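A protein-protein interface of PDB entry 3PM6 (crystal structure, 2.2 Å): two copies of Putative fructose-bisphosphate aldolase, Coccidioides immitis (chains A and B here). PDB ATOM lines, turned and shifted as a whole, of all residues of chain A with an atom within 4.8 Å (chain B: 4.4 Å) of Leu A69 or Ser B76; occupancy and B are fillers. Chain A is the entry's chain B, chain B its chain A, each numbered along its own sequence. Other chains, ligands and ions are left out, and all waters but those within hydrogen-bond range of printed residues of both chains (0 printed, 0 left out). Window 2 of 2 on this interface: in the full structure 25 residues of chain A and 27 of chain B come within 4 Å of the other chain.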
ATOM      1  N   ALA A  66     -15.495 -16.855  -4.677  1.00  0.00           N
ATOM      2  CA  ALA A  66     -16.695 -16.276  -5.269  1.00  0.00           C
ATOM      3  C   ALA A  66     -16.444 -15.422  -6.515  1.00  0.00           C
ATOM      4  O   ALA A  66     -17.332 -14.661  -6.940  1.00  0.00           O
ATOM      5  CB  ALA A  66     -17.434 -15.460  -4.201  1.00  0.00           C
ATOM      6  N   ASP A  67     -15.240 -15.538  -7.088  1.00  0.00           N
ATOM      7  CA  ASP A  67     -14.820 -14.700  -8.215  1.00  0.00           C
ATOM      8  C   ASP A  67     -15.058 -13.245  -7.833  1.00  0.00           C
ATOM      9  O   ASP A  67     -14.627 -12.808  -6.756  1.00  0.00           O
ATOM     10  CB  ASP A  67     -15.527 -15.095  -9.546  1.00  0.00           C
ATOM     11  CG  ASP A  67     -15.166 -16.500 -10.005  1.00  0.00           C
ATOM     12  OD1 ASP A  67     -13.963 -16.867 -10.010  1.00  0.00           O
ATOM     13  OD2 ASP A  67     -16.090 -17.262 -10.353  1.00  0.00           O
ATOM     14  N   SER A  68     -15.762 -12.484  -8.663  1.00  0.00           N
ATOM     15  CA  SER A  68     -15.914 -11.069  -8.335  1.00  0.00           C
ATOM     16  C   SER A  68     -17.105 -10.734  -7.417  1.00  0.00           C
ATOM     17  O   SER A  68     -17.360  -9.562  -7.131  1.00  0.00           O
ATOM     18  CB  SER A  68     -15.921 -10.236  -9.615  1.00  0.00           C
ATOM     19  OG  SER A  68     -17.161 -10.346 -10.277  1.00  0.00           O
ATOM     20  N   LEU A  69     -17.823 -11.745  -6.928  1.00  0.00           N
ATOM     21  CA  LEU A  69     -19.125 -11.495  -6.299  1.00  0.00           C
ATOM     22  C   LEU A  69     -19.080 -10.863  -4.937  1.00  0.00           C
ATOM     23  O   LEU A  69     -19.815  -9.906  -4.695  1.00  0.00           O
ATOM     24  CB  LEU A  69     -19.969 -12.763  -6.183  1.00  0.00           C
ATOM     25  CG  LEU A  69     -20.945 -13.106  -7.295  1.00  0.00           C
ATOM     26  CD1 LEU A  69     -21.760 -14.325  -6.828  1.00  0.00           C
ATOM     27  CD2 LEU A  69     -21.856 -11.904  -7.715  1.00  0.00           C
ATOM     28  N   LEU A  70     -18.283 -11.419  -4.025  1.00  0.00           N
ATOM     29  CA  LEU A  70     -18.067 -10.747  -2.740  1.00  0.00           C
ATOM     30  C   LEU A  70     -17.471  -9.361  -2.948  1.00  0.00           C
ATOM     31  O   LEU A  70     -17.896  -8.396  -2.292  1.00  0.00           O
ATOM     32  CB  LEU A  70     -17.180 -11.556  -1.785  1.00  0.00           C
ATOM     33  CG  LEU A  70     -17.918 -12.588  -0.952  1.00  0.00           C
ATOM     34  CD1 LEU A  70     -16.911 -13.503  -0.246  1.00  0.00           C
ATOM     35  CD2 LEU A  70     -18.773 -11.847   0.059  1.00  0.00           C
ATOM     36  N   VAL A  71     -16.494  -9.258  -3.854  1.00  0.00           N
ATOM     37  CA  VAL A  71     -15.872  -7.960  -4.116  1.00  0.00           C
ATOM     38  C   VAL A  71     -16.890  -6.903  -4.540  1.00  0.00           C
ATOM     39  O   VAL A  71     -16.930  -5.813  -3.957  1.00  0.00           O
ATOM     40  CB  VAL A  71     -14.694  -8.023  -5.159  1.00  0.00           C
ATOM     41  CG1 VAL A  71     -14.128  -6.615  -5.400  1.00  0.00           C
ATOM     42  CG2 VAL A  71     -13.583  -8.986  -4.700  1.00  0.00           C
ATOM     43  N   ARG A  72     -17.700  -7.219  -5.557  1.00  0.00           N
ATOM     44  CA  ARG A  72     -18.617  -6.257  -6.150  1.00  0.00           C
ATOM     45  C   ARG A  72     -19.699  -5.855  -5.183  1.00  0.00           C
ATOM     46  O   ARG A  72     -20.076  -4.691  -5.131  1.00  0.00           O
ATOM     47  CB  ARG A  72     -19.296  -6.802  -7.425  1.00  0.00           C
ATOM     48  CG  ARG A  72     -18.383  -7.021  -8.641  1.00  0.00           C
ATOM     49  CD  ARG A  72     -17.580  -5.775  -9.046  1.00  0.00           C
ATOM     50  NE  ARG A  72     -16.905  -5.993 -10.330  1.00  0.00           N
ATOM     51  CZ  ARG A  72     -16.055  -5.142 -10.908  1.00  0.00           C
ATOM     52  NH1 ARG A  72     -15.743  -3.967 -10.336  1.00  0.00           N
ATOM     53  NH2 ARG A  72     -15.519  -5.483 -12.076  1.00  0.00           N
ATOM     54  N   THR A  73     -20.231  -6.839  -4.457  1.00  0.00           N
ATOM     55  CA  THR A  73     -21.236  -6.589  -3.446  1.00  0.00           C
ATOM     56  C   THR A  73     -20.676  -5.683  -2.311  1.00  0.00           C
ATOM     57  O   THR A  73     -21.293  -4.661  -1.967  1.00  0.00           O
ATOM     58  CB  THR A  73     -21.813  -7.917  -2.922  1.00  0.00           C
ATOM     59  OG1 THR A  73     -22.694  -8.487  -3.912  1.00  0.00           O
ATOM     60  CG2 THR A  73     -22.620  -7.708  -1.669  1.00  0.00           C
ATOM     61  N   GLU A 111     -18.700  -0.340 -12.485  1.00  0.00           N
ATOM     62  CA  GLU A 111     -18.678  -1.249 -11.325  1.00  0.00           C
ATOM     63  C   GLU A 111     -17.433  -1.056 -10.459  1.00  0.00           C
ATOM     64  O   GLU A 111     -16.302  -1.339 -10.896  1.00  0.00           O
ATOM     65  CB  GLU A 111     -18.802  -2.714 -11.755  1.00  0.00           C
ATOM     66  CG  GLU A 111     -20.249  -3.191 -11.967  1.00  0.00           C
ATOM     67  CD  GLU A 111     -20.366  -4.708 -12.017  1.00  0.00           C
ATOM     68  OE1 GLU A 111     -19.578  -5.320 -12.778  1.00  0.00           O
ATOM     69  OE2 GLU A 111     -21.240  -5.292 -11.311  1.00  0.00           O
ATOM     70  N   LEU B  37     -25.395 -16.198   0.179  1.00  0.00           N
ATOM     71  CA  LEU B  37     -24.437 -16.268  -0.915  1.00  0.00           C
ATOM     72  C   LEU B  37     -23.948 -17.695  -1.156  1.00  0.00           C
ATOM     73  O   LEU B  37     -23.731 -18.061  -2.291  1.00  0.00           O
ATOM     74  CB  LEU B  37     -23.242 -15.336  -0.632  1.00  0.00           C
ATOM     75  CG  LEU B  37     -21.966 -15.333  -1.478  1.00  0.00           C
ATOM     76  CD1 LEU B  37     -22.241 -15.260  -2.948  1.00  0.00           C
ATOM     77  CD2 LEU B  37     -21.138 -14.134  -1.084  1.00  0.00           C
ATOM     78  N   LEU B  41     -24.100 -19.382  -4.823  1.00  0.00           N
ATOM     79  CA  LEU B  41     -22.928 -19.983  -5.475  1.00  0.00           C
ATOM     80  C   LEU B  41     -23.199 -21.437  -5.795  1.00  0.00           C
ATOM     81  O   LEU B  41     -22.861 -21.894  -6.893  1.00  0.00           O
ATOM     82  CB  LEU B  41     -21.672 -19.868  -4.602  1.00  0.00           C
ATOM     83  CG  LEU B  41     -21.101 -18.455  -4.617  1.00  0.00           C
ATOM     84  CD1 LEU B  41     -19.879 -18.335  -3.709  1.00  0.00           C
ATOM     85  CD2 LEU B  41     -20.751 -18.050  -6.056  1.00  0.00           C
ATOM     86  N   ARG B  72     -29.130  -7.876  -5.229  1.00  0.00           N
ATOM     87  CA  ARG B  72     -28.102  -7.374  -6.138  1.00  0.00           C
ATOM     88  C   ARG B  72     -27.025  -8.435  -6.404  1.00  0.00           C
ATOM     89  O   ARG B  72     -26.622  -8.644  -7.540  1.00  0.00           O
ATOM     90  CB  ARG B  72     -27.456  -6.093  -5.574  1.00  0.00           C
ATOM     91  N   THR B  73     -26.562  -9.090  -5.350  1.00  0.00           N
ATOM     92  CA  THR B  73     -25.629 -10.209  -5.472  1.00  0.00           C
ATOM     93  C   THR B  73     -26.197 -11.307  -6.364  1.00  0.00           C
ATOM     94  O   THR B  73     -25.535 -11.744  -7.281  1.00  0.00           O
ATOM     95  CB  THR B  73     -25.318 -10.818  -4.106  1.00  0.00           C
ATOM     96  OG1 THR B  73     -24.895  -9.771  -3.219  1.00  0.00           O
ATOM     97  CG2 THR B  73     -24.216 -11.878  -4.223  1.00  0.00           C
ATOM     98  N   ALA B  74     -27.432 -11.735  -6.100  1.00  0.00           N
ATOM     99  CA  ALA B  74     -28.080 -12.811  -6.900  1.00  0.00           C
ATOM    100  C   ALA B  74     -28.348 -12.389  -8.332  1.00  0.00           C
ATOM    101  O   ALA B  74     -28.152 -13.184  -9.261  1.00  0.00           O
ATOM    102  CB  ALA B  74     -29.375 -13.313  -6.236  1.00  0.00           C
ATOM    103  N   ALA B  75     -28.809 -11.153  -8.523  1.00  0.00           N
ATOM    104  CA  ALA B  75     -29.154 -10.704  -9.893  1.00  0.00           C
ATOM    105  C   ALA B  75     -27.884 -10.673 -10.735  1.00  0.00           C
ATOM    106  O   ALA B  75     -27.873 -11.073 -11.917  1.00  0.00           O
ATOM    107  CB  ALA B  75     -29.811  -9.327  -9.892  1.00  0.00           C
ATOM    108  N   SER B  76     -26.813 -10.221 -10.098  1.00  0.00           N
ATOM    109  CA  SER B  76     -25.531 -10.124 -10.754  1.00  0.00           C
ATOM    110  C   SER B  76     -24.963 -11.514 -11.070  1.00  0.00           C
ATOM    111  O   SER B  76     -24.575 -11.771 -12.206  1.00  0.00           O
ATOM    112  CB  SER B  76     -24.572  -9.291  -9.888  1.00  0.00           C
ATOM    113  OG  SER B  76     -23.284  -9.381 -10.422  1.00  0.00           O
ATOM    114  N   ALA B  77     -24.946 -12.417 -10.088  1.00  0.00           N
ATOM    115  CA  ALA B  77     -24.560 -13.803 -10.345  1.00  0.00           C
ATOM    116  C   ALA B  77     -25.328 -14.404 -11.543  1.00  0.00           C
ATOM    117  O   ALA B  77     -24.734 -15.133 -12.346  1.00  0.00           O
ATOM    118  CB  ALA B  77     -24.750 -14.666  -9.095  1.00  0.00           C
ATOM    119  N   CYS B  78     -26.631 -14.099 -11.645  1.00  0.00           N
ATOM    120  CA  CYS B  78     -27.477 -14.582 -12.745  1.00  0.00           C
ATOM    121  C   CYS B  78     -26.945 -14.161 -14.106  1.00  0.00           C
ATOM    122  O   CYS B  78     -26.806 -15.002 -15.000  1.00  0.00           O
ATOM    123  CB  CYS B  78     -28.940 -14.076 -12.613  1.00  0.00           C
ATOM    124  SG  CYS B  78     -29.898 -14.901 -11.383  1.00  0.00           S
ATOM    125  N   ARG B  79     -26.699 -12.855 -14.250  1.00  0.00           N
ATOM    126  CA  ARG B  79     -26.181 -12.240 -15.471  1.00  0.00           C
ATOM    127  C   ARG B  79     -24.862 -12.839 -15.920  1.00  0.00           C
ATOM    128  O   ARG B  79     -24.686 -13.073 -17.103  1.00  0.00           O
ATOM    129  CB  ARG B  79     -25.987 -10.722 -15.315  1.00  0.00           C
ATOM    130  CG  ARG B  79     -27.268  -9.911 -15.032  1.00  0.00           C
ATOM    131  CD  ARG B  79     -28.339 -10.067 -16.113  1.00  0.00           C
ATOM    132  NE  ARG B  79     -29.689  -9.801 -15.600  1.00  0.00           N
ATOM    133  CZ  ARG B  79     -30.465  -8.775 -15.961  1.00  0.00           C
ATOM    134  NH1 ARG B  79     -30.035  -7.870 -16.844  1.00  0.00           N
ATOM    135  NH2 ARG B  79     -31.687  -8.653 -15.435  1.00  0.00           N
ATOM    136  N   ALA B  80     -23.959 -13.088 -14.971  1.00  0.00           N
ATOM    137  CA  ALA B  80     -22.605 -13.545 -15.260  1.00  0.00           C
ATOM    138  C   ALA B  80     -22.500 -15.046 -15.555  1.00  0.00           C
ATOM    139  O   ALA B  80     -21.440 -15.526 -15.977  1.00  0.00           O
ATOM    140  CB  ALA B  80     -21.674 -13.176 -14.104  1.00  0.00           C
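The side-chain hydroxyl (OG1) of Thr A73 is in hydrogen-bond range of the side-chain hydroxyl (OG1) of Thr B73.
The backbone carbonyl oxygen (O) of Leu A69 lies within hydrogen-bond range of the side-chain hydroxyl (OG1) of Thr A73 (3.3 Å).
Among the printed residues, merely in contact across the chains: Leu A70 with Leu B37, Leu A69 with Thr B73, Leu A69 with Ala B77, Ala A66 with Leu B41, Leu A69 with Leu B41 and Leu A69 with Ser B76.
Of the printed residues of chain B, Ala A66 touches Leu B41 (3.8 Å). Of the printed residues of chain B, Leu A69 touches Leu B41, Thr B73, Ser B76 and Ala B77. Of the printed residues of chain A, Leu B41 touches Ala A66 and Leu A69. Ser B76 touches one residue of chain A. Printed residues of chain A within 4 Å of Ala B77: Leu A69 (3.8 Å). Arg B79 touches none of the printed residues of chain A.
Printed residues of chain A that touch a printed residue of chain B: Ala A66, Leu A69, Leu A70 and Thr A73. Of the 11 printed residues of chain B, 5 touch a printed residue of chain A.
Thr A73 touches its own counterpart, Thr B73. Positions printed for both chains: 72 and 73. Of the 7 pairs that touch across the chains among the printed residues, 1 has its exchanged pair printed and touching as well.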
